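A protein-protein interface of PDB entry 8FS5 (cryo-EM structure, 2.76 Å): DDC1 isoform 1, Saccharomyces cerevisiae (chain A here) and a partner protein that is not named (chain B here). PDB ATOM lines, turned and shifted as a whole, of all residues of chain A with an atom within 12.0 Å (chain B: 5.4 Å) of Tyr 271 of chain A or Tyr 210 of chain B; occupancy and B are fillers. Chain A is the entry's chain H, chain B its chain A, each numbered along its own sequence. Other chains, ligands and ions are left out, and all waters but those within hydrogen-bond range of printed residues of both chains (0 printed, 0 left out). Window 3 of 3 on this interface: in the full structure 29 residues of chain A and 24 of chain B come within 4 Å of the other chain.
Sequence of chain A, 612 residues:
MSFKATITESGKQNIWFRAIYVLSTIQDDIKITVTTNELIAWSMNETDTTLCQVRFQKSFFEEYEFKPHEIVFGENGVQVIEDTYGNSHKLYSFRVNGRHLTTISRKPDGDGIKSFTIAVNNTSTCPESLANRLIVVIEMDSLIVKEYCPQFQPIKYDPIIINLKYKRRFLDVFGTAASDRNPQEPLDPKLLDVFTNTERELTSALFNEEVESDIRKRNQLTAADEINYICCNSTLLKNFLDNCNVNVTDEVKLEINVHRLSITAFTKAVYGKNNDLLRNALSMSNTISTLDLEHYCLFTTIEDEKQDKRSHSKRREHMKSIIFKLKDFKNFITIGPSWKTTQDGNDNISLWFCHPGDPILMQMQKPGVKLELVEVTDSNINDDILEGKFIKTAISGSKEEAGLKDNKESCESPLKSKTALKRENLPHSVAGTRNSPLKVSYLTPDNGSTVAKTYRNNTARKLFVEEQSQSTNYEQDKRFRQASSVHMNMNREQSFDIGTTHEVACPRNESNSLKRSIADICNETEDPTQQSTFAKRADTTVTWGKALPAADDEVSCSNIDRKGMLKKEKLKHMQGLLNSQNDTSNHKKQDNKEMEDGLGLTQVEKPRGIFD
Tyr 271 of chain A touches just one residue of chain B: Tyr 210 (3.2 Å).
Printed residues of chain A within 4 Å of Tyr 210 of chain B: Val 270, Tyr 271, Lys 273 and Leu 278.
Of chain A, only Leu 278 comes within 4 Å of Leu 206 of chain B.
No residue of chain A comes within 4 Å of Leu 209 of chain B.
No residue of chain A comes within 4 Å of Ser 211 of chain B.
Ser 212 of chain B touches just one residue of chain A: Lys 268 (2.7 Å).
Of the printed residues of chain A, Glu 253 of chain B touches Lys 273 (3.8 Å).
Of the printed residues of chain B, Leu 278 of chain A touches Leu 206 and Tyr 210.
Of the printed residues of chain B, Arg 279 of chain A touches Gln 207 (3.2 Å).
Of the printed residues of chain B, Lys 273 of chain A touches Tyr 210 (3.9 Å) and Glu 253 (3.8 Å).
Of the printed residues of chain B, Lys 268 of chain A touches Ser 212 (2.7 Å).
Among the printed residues, merely in contact across the chains: Arg 279 of chain A with Gln 207 of chain B (3.2 Å), Tyr 271 of chain A with Tyr 210 of chain B (3.2 Å), Val 270 of chain A with Tyr 210 of chain B (3.4 Å), Leu 278 of chain A with Tyr 210 of chain B (3.8 Å), Leu 278 of chain A with Leu 206 of chain B (3.8 Å), Lys 273 of chain A with Glu 253 of chain B (3.8 Å), Lys 273 of chain A with Tyr 210 of chain B (3.9 Å) and Val 270 of chain A with Gln 207 of chain B (3.9 Å).
NZ of Lys 268 of chain A sits at hydrogen-bond distance from OG of Ser 212 of chain B (2.7 Å).
Printed residues of chain A that touch a printed residue of chain B: Lys 268, Val 270, Tyr 271, Lys 273, Leu 278 and Arg 279.
Hydrophobic or aromatic side chains of chain A within 4 Å of the printed part of chain B: Val 270 and Leu 278.
Along chain B the printed residues that touch a printed residue of chain A span positions 206 to 253.
Among the printed residues, no Asp or Glu carboxylate lies within 4 Å of a Lys or Arg side-chain nitrogen of the other chain.
The backbone carbonyl oxygen of Val 270 of chain A sits at hydrogen-bond distance from the backbone NH of Leu 278 of chain A, 2.9 Å away.
The backbone carbonyl oxygen (O) of Arg 279 of chain A is in hydrogen-bond range of the backbone NH (N) of Val 270 of chain A (3.2 Å).
The side-chain hydroxyl (OG1) of Thr 267 of chain A is in hydrogen-bond range of the guanidinium group (NH2) of Arg 279 of chain A (2.6 Å).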
ATOM      1  N   PHE A 266     -11.748 -19.010   6.768  1.00  0.00           N
ATOM      2  CA  PHE A 266     -13.036 -19.013   6.096  1.00  0.00           C
ATOM      3  C   PHE A 266     -14.157 -19.188   7.112  1.00  0.00           C
ATOM      4  O   PHE A 266     -13.941 -19.603   8.253  1.00  0.00           O
ATOM      5  CB  PHE A 266     -13.107 -20.128   5.044  1.00  0.00           C
ATOM      6  CG  PHE A 266     -13.084 -21.514   5.627  1.00  0.00           C
ATOM      7  CD1 PHE A 266     -11.885 -22.121   5.963  1.00  0.00           C
ATOM      8  CD2 PHE A 266     -14.264 -22.213   5.830  1.00  0.00           C
ATOM      9  CE1 PHE A 266     -11.866 -23.393   6.501  1.00  0.00           C
ATOM     10  CE2 PHE A 266     -14.249 -23.485   6.366  1.00  0.00           C
ATOM     11  CZ  PHE A 266     -13.049 -24.075   6.701  1.00  0.00           C
ATOM     12  N   THR A 267     -15.369 -18.860   6.676  1.00  0.00           N
ATOM     13  CA  THR A 267     -16.573 -19.178   7.434  1.00  0.00           C
ATOM     14  C   THR A 267     -17.624 -19.664   6.450  1.00  0.00           C
ATOM     15  O   THR A 267     -17.609 -19.268   5.280  1.00  0.00           O
ATOM     16  CB  THR A 267     -17.072 -17.972   8.239  1.00  0.00           C
ATOM     17  OG1 THR A 267     -18.046 -18.404   9.197  1.00  0.00           O
ATOM     18  CG2 THR A 267     -17.687 -16.912   7.336  1.00  0.00           C
ATOM     19  N   LYS A 268     -18.509 -20.545   6.907  1.00  0.00           N
ATOM     20  CA  LYS A 268     -19.496 -21.123   6.012  1.00  0.00           C
ATOM     21  C   LYS A 268     -20.782 -20.301   6.017  1.00  0.00           C
ATOM     22  O   LYS A 268     -21.037 -19.493   6.915  1.00  0.00           O
ATOM     23  CB  LYS A 268     -19.792 -22.572   6.401  1.00  0.00           C
ATOM     24  CG  LYS A 268     -19.079 -23.594   5.531  1.00  0.00           C
ATOM     25  CD  LYS A 268     -18.693 -24.826   6.329  1.00  0.00           C
ATOM     26  CE  LYS A 268     -19.910 -25.682   6.631  1.00  0.00           C
ATOM     27  NZ  LYS A 268     -20.816 -25.791   5.454  1.00  0.00           N
ATOM     28  N   ALA A 269     -21.596 -20.521   4.991  1.00  0.00           N
ATOM     29  CA  ALA A 269     -22.860 -19.819   4.825  1.00  0.00           C
ATOM     30  C   ALA A 269     -24.016 -20.715   5.248  1.00  0.00           C
ATOM     31  O   ALA A 269     -24.055 -21.900   4.906  1.00  0.00           O
ATOM     32  CB  ALA A 269     -23.050 -19.371   3.375  1.00  0.00           C
ATOM     33  N   VAL A 270     -24.955 -20.141   5.994  1.00  0.00           N
ATOM     34  CA  VAL A 270     -26.137 -20.848   6.472  1.00  0.00           C
ATOM     35  C   VAL A 270     -27.336 -20.320   5.698  1.00  0.00           C
ATOM     36  O   VAL A 270     -27.571 -19.106   5.656  1.00  0.00           O
ATOM     37  CB  VAL A 270     -26.329 -20.673   7.987  1.00  0.00           C
ATOM     38  CG1 VAL A 270     -27.628 -21.323   8.436  1.00  0.00           C
ATOM     39  CG2 VAL A 270     -25.144 -21.256   8.741  1.00  0.00           C
ATOM     40  N   TYR A 271     -28.092 -21.227   5.088  1.00  0.00           N
ATOM     41  CA  TYR A 271     -29.219 -20.868   4.238  1.00  0.00           C
ATOM     42  C   TYR A 271     -30.525 -21.085   4.992  1.00  0.00           C
ATOM     43  O   TYR A 271     -30.726 -22.136   5.608  1.00  0.00           O
ATOM     44  CB  TYR A 271     -29.204 -21.684   2.946  1.00  0.00           C
ATOM     45  CG  TYR A 271     -27.929 -21.514   2.148  1.00  0.00           C
ATOM     46  CD1 TYR A 271     -27.694 -20.357   1.417  1.00  0.00           C
ATOM     47  CD2 TYR A 271     -26.959 -22.508   2.134  1.00  0.00           C
ATOM     48  CE1 TYR A 271     -26.531 -20.195   0.690  1.00  0.00           C
ATOM     49  CE2 TYR A 271     -25.792 -22.355   1.408  1.00  0.00           C
ATOM     50  CZ  TYR A 271     -25.583 -21.197   0.689  1.00  0.00           C
ATOM     51  OH  TYR A 271     -24.423 -21.039  -0.035  1.00  0.00           O
ATOM     52  N   GLY A 272     -31.410 -20.091   4.931  1.00  0.00           N
ATOM     53  CA  GLY A 272     -32.642 -20.111   5.697  1.00  0.00           C
ATOM     54  C   GLY A 272     -33.787 -20.848   5.035  1.00  0.00           C
ATOM     55  O   GLY A 272     -33.569 -21.773   4.246  1.00  0.00           O
ATOM     56  N   LYS A 273     -35.017 -20.448   5.362  1.00  0.00           N
ATOM     57  CA  LYS A 273     -36.218 -21.111   4.864  1.00  0.00           C
ATOM     58  C   LYS A 273     -36.337 -21.014   3.347  1.00  0.00           C
ATOM     59  O   LYS A 273     -36.239 -22.026   2.646  1.00  0.00           O
ATOM     60  CB  LYS A 273     -37.460 -20.510   5.525  1.00  0.00           C
ATOM     61  CG  LYS A 273     -38.772 -21.130   5.074  1.00  0.00           C
ATOM     62  CD  LYS A 273     -39.942 -20.570   5.865  1.00  0.00           C
ATOM     63  CE  LYS A 273     -39.823 -20.905   7.342  1.00  0.00           C
ATOM     64  NZ  LYS A 273     -41.066 -20.565   8.089  1.00  0.00           N
ATOM     65  N   ASN A 274     -36.545 -19.803   2.832  1.00  0.00           N
ATOM     66  CA  ASN A 274     -36.636 -19.600   1.390  1.00  0.00           C
ATOM     67  C   ASN A 274     -35.270 -19.247   0.821  1.00  0.00           C
ATOM     68  O   ASN A 274     -35.125 -18.239   0.121  1.00  0.00           O
ATOM     69  CB  ASN A 274     -37.652 -18.503   1.062  1.00  0.00           C
ATOM     70  CG  ASN A 274     -38.996 -18.737   1.723  1.00  0.00           C
ATOM     71  OD1 ASN A 274     -39.385 -19.876   1.980  1.00  0.00           O
ATOM     72  ND2 ASN A 274     -39.716 -17.655   2.000  1.00  0.00           N
ATOM     73  N   ASN A 275     -34.269 -20.081   1.119  1.00  0.00           N
ATOM     74  CA  ASN A 275     -32.878 -19.847   0.723  1.00  0.00           C
ATOM     75  C   ASN A 275     -32.388 -18.483   1.209  1.00  0.00           C
ATOM     76  O   ASN A 275     -31.590 -17.816   0.546  1.00  0.00           O
ATOM     77  CB  ASN A 275     -32.698 -19.990  -0.792  1.00  0.00           C
ATOM     78  CG  ASN A 275     -31.294 -20.424  -1.178  1.00  0.00           C
ATOM     79  OD1 ASN A 275     -30.346 -19.639  -1.126  1.00  0.00           O
ATOM     80  ND2 ASN A 275     -31.153 -21.686  -1.565  1.00  0.00           N
ATOM     81  N   ASP A 276     -32.879 -18.054   2.369  1.00  0.00           N
ATOM     82  CA  ASP A 276     -32.447 -16.791   2.945  1.00  0.00           C
ATOM     83  C   ASP A 276     -31.055 -16.941   3.555  1.00  0.00           C
ATOM     84  O   ASP A 276     -30.655 -18.015   4.009  1.00  0.00           O
ATOM     85  CB  ASP A 276     -33.447 -16.314   3.998  1.00  0.00           C
ATOM     86  CG  ASP A 276     -33.414 -14.811   4.193  1.00  0.00           C
ATOM     87  OD1 ASP A 276     -32.549 -14.327   4.952  1.00  0.00           O
ATOM     88  OD2 ASP A 276     -34.255 -14.113   3.586  1.00  0.00           O
ATOM     89  N   LEU A 277     -30.315 -15.839   3.570  1.00  0.00           N
ATOM     90  CA  LEU A 277     -28.928 -15.831   4.028  1.00  0.00           C
ATOM     91  C   LEU A 277     -28.915 -15.551   5.527  1.00  0.00           C
ATOM     92  O   LEU A 277     -28.859 -14.395   5.952  1.00  0.00           O
ATOM     93  CB  LEU A 277     -28.109 -14.796   3.260  1.00  0.00           C
ATOM     94  CG  LEU A 277     -26.590 -14.970   3.326  1.00  0.00           C
ATOM     95  CD1 LEU A 277     -26.185 -16.329   2.777  1.00  0.00           C
ATOM     96  CD2 LEU A 277     -25.888 -13.852   2.571  1.00  0.00           C
ATOM     97  N   LEU A 278     -28.975 -16.620   6.326  1.00  0.00           N
ATOM     98  CA  LEU A 278     -28.844 -16.467   7.772  1.00  0.00           C
ATOM     99  C   LEU A 278     -27.441 -16.011   8.150  1.00  0.00           C
ATOM    100  O   LEU A 278     -27.272 -15.192   9.060  1.00  0.00           O
ATOM    101  CB  LEU A 278     -29.192 -17.780   8.474  1.00  0.00           C
ATOM    102  CG  LEU A 278     -30.647 -18.243   8.376  1.00  0.00           C
ATOM    103  CD1 LEU A 278     -30.842 -19.564   9.104  1.00  0.00           C
ATOM    104  CD2 LEU A 278     -31.586 -17.181   8.925  1.00  0.00           C
ATOM    105  N   ARG A 279     -26.425 -16.531   7.464  1.00  0.00           N
ATOM    106  CA  ARG A 279     -25.040 -16.162   7.717  1.00  0.00           C
ATOM    107  C   ARG A 279     -24.278 -16.135   6.401  1.00  0.00           C
ATOM    108  O   ARG A 279     -24.474 -17.002   5.544  1.00  0.00           O
ATOM    109  CB  ARG A 279     -24.374 -17.137   8.695  1.00  0.00           C
ATOM    110  CG  ARG A 279     -23.042 -16.655   9.237  1.00  0.00           C
ATOM    111  CD  ARG A 279     -22.780 -17.216  10.622  1.00  0.00           C
ATOM    112  NE  ARG A 279     -21.393 -17.038  11.028  1.00  0.00           N
ATOM    113  CZ  ARG A 279     -20.470 -17.988  10.971  1.00  0.00           C
ATOM    114  NH1 ARG A 279     -20.757 -19.205  10.540  1.00  0.00           N
ATOM    115  NH2 ARG A 279     -19.228 -17.708  11.351  1.00  0.00           N
ATOM    116  N   ASN A 280     -23.410 -15.138   6.248  1.00  0.00           N
ATOM    117  CA  ASN A 280     -22.626 -14.973   5.037  1.00  0.00           C
ATOM    118  C   ASN A 280     -21.389 -15.870   5.081  1.00  0.00           C
ATOM    119  O   ASN A 280     -21.180 -16.644   6.018  1.00  0.00           O
ATOM    120  CB  ASN A 280     -22.239 -13.507   4.851  1.00  0.00           C
ATOM    121  CG  ASN A 280     -23.346 -12.556   5.263  1.00  0.00           C
ATOM    122  OD1 ASN A 280     -23.776 -12.549   6.416  1.00  0.00           O
ATOM    123  ND2 ASN A 280     -23.812 -11.746   4.320  1.00  0.00           N
ATOM    124  N   ALA A 281     -20.554 -15.766   4.047  1.00  0.00           N
ATOM    125  CA  ALA A 281     -19.345 -16.580   3.921  1.00  0.00           C
ATOM    126  C   ALA A 281     -18.192 -15.689   3.469  1.00  0.00           C
ATOM    127  O   ALA A 281     -18.169 -15.222   2.326  1.00  0.00           O
ATOM    128  CB  ALA A 281     -19.564 -17.736   2.949  1.00  0.00           C
ATOM    129  N   LEU A 282     -17.240 -15.456   4.366  1.00  0.00           N
ATOM    130  CA  LEU A 282     -16.021 -14.722   4.059  1.00  0.00           C
ATOM    131  C   LEU A 282     -14.852 -15.699   4.025  1.00  0.00           C
ATOM    132  O   LEU A 282     -14.711 -16.541   4.916  1.00  0.00           O
ATOM    133  CB  LEU A 282     -15.769 -13.622   5.094  1.00  0.00           C
ATOM    134  CG  LEU A 282     -14.680 -12.580   4.824  1.00  0.00           C
ATOM    135  CD1 LEU A 282     -14.519 -12.304   3.335  1.00  0.00           C
ATOM    136  CD2 LEU A 282     -14.982 -11.293   5.578  1.00  0.00           C
ATOM    137  N   SER A 283     -14.013 -15.582   2.994  1.00  0.00           N
ATOM    138  CA  SER A 283     -12.977 -16.572   2.704  1.00  0.00           C
ATOM    139  C   SER A 283     -11.626 -15.883   2.495  1.00  0.00           C
ATOM    140  O   SER A 283     -10.926 -16.125   1.512  1.00  0.00           O
ATOM    141  CB  SER A 283     -13.355 -17.415   1.487  1.00  0.00           C
ATOM    142  OG  SER A 283     -12.484 -18.523   1.342  1.00  0.00           O
ATOM    143  N   ARG B 103     -32.499 -32.934  14.161  1.00  0.00           N
ATOM    144  CA  ARG B 103     -31.225 -32.379  14.601  1.00  0.00           C
ATOM    145  C   ARG B 103     -31.219 -31.970  16.064  1.00  0.00           C
ATOM    146  O   ARG B 103     -30.214 -32.170  16.749  1.00  0.00           O
ATOM    147  CB  ARG B 103     -30.852 -31.169  13.737  1.00  0.00           C
ATOM    148  CG  ARG B 103     -29.568 -31.346  12.944  1.00  0.00           C
ATOM    149  CD  ARG B 103     -29.504 -30.375  11.777  1.00  0.00           C
ATOM    150  NE  ARG B 103     -28.557 -30.809  10.757  1.00  0.00           N
ATOM    151  CZ  ARG B 103     -28.022 -30.010   9.844  1.00  0.00           C
ATOM    152  NH1 ARG B 103     -28.326 -28.724   9.788  1.00  0.00           N
ATOM    153  NH2 ARG B 103     -27.164 -30.516   8.962  1.00  0.00           N
ATOM    154  N   ILE B 205     -29.659 -21.058  17.300  1.00  0.00           N
ATOM    155  CA  ILE B 205     -30.345 -22.333  17.120  1.00  0.00           C
ATOM    156  C   ILE B 205     -30.831 -22.497  15.684  1.00  0.00           C
ATOM    157  O   ILE B 205     -30.726 -23.583  15.107  1.00  0.00           O
ATOM    158  CB  ILE B 205     -31.504 -22.452  18.128  1.00  0.00           C
ATOM    159  CG1 ILE B 205     -30.954 -22.653  19.539  1.00  0.00           C
ATOM    160  CG2 ILE B 205     -32.437 -23.593  17.753  1.00  0.00           C
ATOM    161  CD1 ILE B 205     -32.008 -23.002  20.547  1.00  0.00           C
ATOM    162  N   LEU B 206     -31.362 -21.423  15.093  1.00  0.00           N
ATOM    163  CA  LEU B 206     -31.790 -21.477  13.699  1.00  0.00           C
ATOM    164  C   LEU B 206     -30.616 -21.720  12.759  1.00  0.00           C
ATOM    165  O   LEU B 206     -30.784 -22.353  11.711  1.00  0.00           O
ATOM    166  CB  LEU B 206     -32.512 -20.186  13.317  1.00  0.00           C
ATOM    167  CG  LEU B 206     -33.999 -20.133  13.662  1.00  0.00           C
ATOM    168  CD1 LEU B 206     -34.545 -18.722  13.504  1.00  0.00           C
ATOM    169  CD2 LEU B 206     -34.775 -21.119  12.804  1.00  0.00           C
ATOM    170  N   GLN B 207     -29.431 -21.235  13.115  1.00  0.00           N
ATOM    171  CA  GLN B 207     -28.223 -21.467  12.331  1.00  0.00           C
ATOM    172  C   GLN B 207     -27.681 -22.876  12.492  1.00  0.00           C
ATOM    173  O   GLN B 207     -26.814 -23.293  11.711  1.00  0.00           O
ATOM    174  CB  GLN B 207     -27.156 -20.443  12.720  1.00  0.00           C
ATOM    175  CG  GLN B 207     -27.197 -19.170  11.896  1.00  0.00           C
ATOM    176  CD  GLN B 207     -26.232 -18.121  12.406  1.00  0.00           C
ATOM    177  OE1 GLN B 207     -25.041 -18.384  12.563  1.00  0.00           O
ATOM    178  NE2 GLN B 207     -26.743 -16.924  12.666  1.00  0.00           N
ATOM    179  N   TRP B 208     -28.174 -23.611  13.485  1.00  0.00           N
ATOM    180  CA  TRP B 208     -27.855 -25.020  13.672  1.00  0.00           C
ATOM    181  C   TRP B 208     -28.870 -25.926  12.993  1.00  0.00           C
ATOM    182  O   TRP B 208     -28.499 -26.958  12.426  1.00  0.00           O
ATOM    183  CB  TRP B 208     -27.774 -25.344  15.174  1.00  0.00           C
ATOM    184  CG  TRP B 208     -27.385 -26.763  15.493  1.00  0.00           C
ATOM    185  CD1 TRP B 208     -28.180 -27.872  15.421  1.00  0.00           C
ATOM    186  CD2 TRP B 208     -26.104 -27.219  15.944  1.00  0.00           C
ATOM    187  NE1 TRP B 208     -27.473 -28.988  15.794  1.00  0.00           N
ATOM    188  CE2 TRP B 208     -26.195 -28.615  16.120  1.00  0.00           C
ATOM    189  CE3 TRP B 208     -24.888 -26.584  16.214  1.00  0.00           C
ATOM    190  CZ2 TRP B 208     -25.117 -29.384  16.554  1.00  0.00           C
ATOM    191  CZ3 TRP B 208     -23.820 -27.349  16.643  1.00  0.00           C
ATOM    192  CH2 TRP B 208     -23.941 -28.735  16.809  1.00  0.00           C
ATOM    193  N   LEU B 209     -30.153 -25.561  13.046  1.00  0.00           N
ATOM    194  CA  LEU B 209     -31.172 -26.326  12.333  1.00  0.00           C
ATOM    195  C   LEU B 209     -31.003 -26.211  10.823  1.00  0.00           C
ATOM    196  O   LEU B 209     -31.237 -27.184  10.096  1.00  0.00           O
ATOM    197  CB  LEU B 209     -32.568 -25.856  12.744  1.00  0.00           C
ATOM    198  CG  LEU B 209     -33.116 -26.394  14.065  1.00  0.00           C
ATOM    199  CD1 LEU B 209     -34.363 -25.630  14.480  1.00  0.00           C
ATOM    200  CD2 LEU B 209     -33.407 -27.883  13.955  1.00  0.00           C
ATOM    201  N   TYR B 210     -30.601 -25.037  10.336  1.00  0.00           N
ATOM    202  CA  TYR B 210     -30.431 -24.785   8.911  1.00  0.00           C
ATOM    203  C   TYR B 210     -28.971 -24.906   8.480  1.00  0.00           C
ATOM    204  O   TYR B 210     -28.584 -24.393   7.428  1.00  0.00           O
ATOM    205  CB  TYR B 210     -30.977 -23.406   8.547  1.00  0.00           C
ATOM    206  CG  TYR B 210     -32.485 -23.335   8.471  1.00  0.00           C
ATOM    207  CD1 TYR B 210     -33.186 -24.065   7.519  1.00  0.00           C
ATOM    208  CD2 TYR B 210     -33.207 -22.534   9.346  1.00  0.00           C
ATOM    209  CE1 TYR B 210     -34.565 -24.002   7.444  1.00  0.00           C
ATOM    210  CE2 TYR B 210     -34.586 -22.464   9.278  1.00  0.00           C
ATOM    211  CZ  TYR B 210     -35.259 -23.200   8.325  1.00  0.00           C
ATOM    212  OH  TYR B 210     -36.632 -23.134   8.255  1.00  0.00           O
ATOM    213  N   SER B 211     -28.154 -25.579   9.285  1.00  0.00           N
ATOM    214  CA  SER B 211     -26.737 -25.733   8.995  1.00  0.00           C
ATOM    215  C   SER B 211     -26.531 -26.667   7.810  1.00  0.00           C
ATOM    216  O   SER B 211     -27.267 -27.642   7.634  1.00  0.00           O
ATOM    217  CB  SER B 211     -25.992 -26.271  10.218  1.00  0.00           C
ATOM    218  OG  SER B 211     -24.711 -26.758   9.860  1.00  0.00           O
ATOM    219  N   SER B 212     -25.521 -26.358   6.996  1.00  0.00           N
ATOM    220  CA  SER B 212     -25.195 -27.170   5.832  1.00  0.00           C
ATOM    221  C   SER B 212     -24.116 -28.207   6.114  1.00  0.00           C
ATOM    222  O   SER B 212     -23.619 -28.828   5.167  1.00  0.00           O
ATOM    223  CB  SER B 212     -24.754 -26.274   4.672  1.00  0.00           C
ATOM    224  OG  SER B 212     -23.346 -26.116   4.656  1.00  0.00           O
ATOM    225  N   GLU B 253     -40.560 -20.639  14.150  1.00  0.00           N
ATOM    226  CA  GLU B 253     -39.689 -21.252  13.152  1.00  0.00           C
ATOM    227  C   GLU B 253     -38.901 -22.408  13.755  1.00  0.00           C
ATOM    228  O   GLU B 253     -38.756 -23.469  13.135  1.00  0.00           O
ATOM    229  CB  GLU B 253     -38.749 -20.201  12.559  1.00  0.00           C
ATOM    230  CG  GLU B 253     -38.046 -20.647  11.287  1.00  0.00           C
ATOM    231  CD  GLU B 253     -37.309 -19.513  10.602  1.00  0.00           C
ATOM    232  OE1 GLU B 253     -37.170 -18.434  11.218  1.00  0.00           O
ATOM    233  OE2 GLU B 253     -36.869 -19.699   9.448  1.00  0.00           O
ATOM    234  N   HIS B 257     -40.047 -26.686  13.140  1.00  0.00           N
ATOM    235  CA  HIS B 257     -39.001 -27.018  12.190  1.00  0.00           C
ATOM    236  C   HIS B 257     -39.014 -28.512  11.888  1.00  0.00           C
ATOM    237  O   HIS B 257     -39.241 -29.323  12.793  1.00  0.00           O
ATOM    238  CB  HIS B 257     -37.622 -26.620  12.730  1.00  0.00           C
ATOM    239  CG  HIS B 257     -36.573 -26.478  11.672  1.00  0.00           C
ATOM    240  ND1 HIS B 257     -35.904 -27.558  11.138  1.00  0.00           N
ATOM    241  CD2 HIS B 257     -36.080 -25.383  11.047  1.00  0.00           C
ATOM    242  CE1 HIS B 257     -35.042 -27.134  10.230  1.00  0.00           C
ATOM    243  NE2 HIS B 257     -35.129 -25.818  10.155  1.00  0.00           N
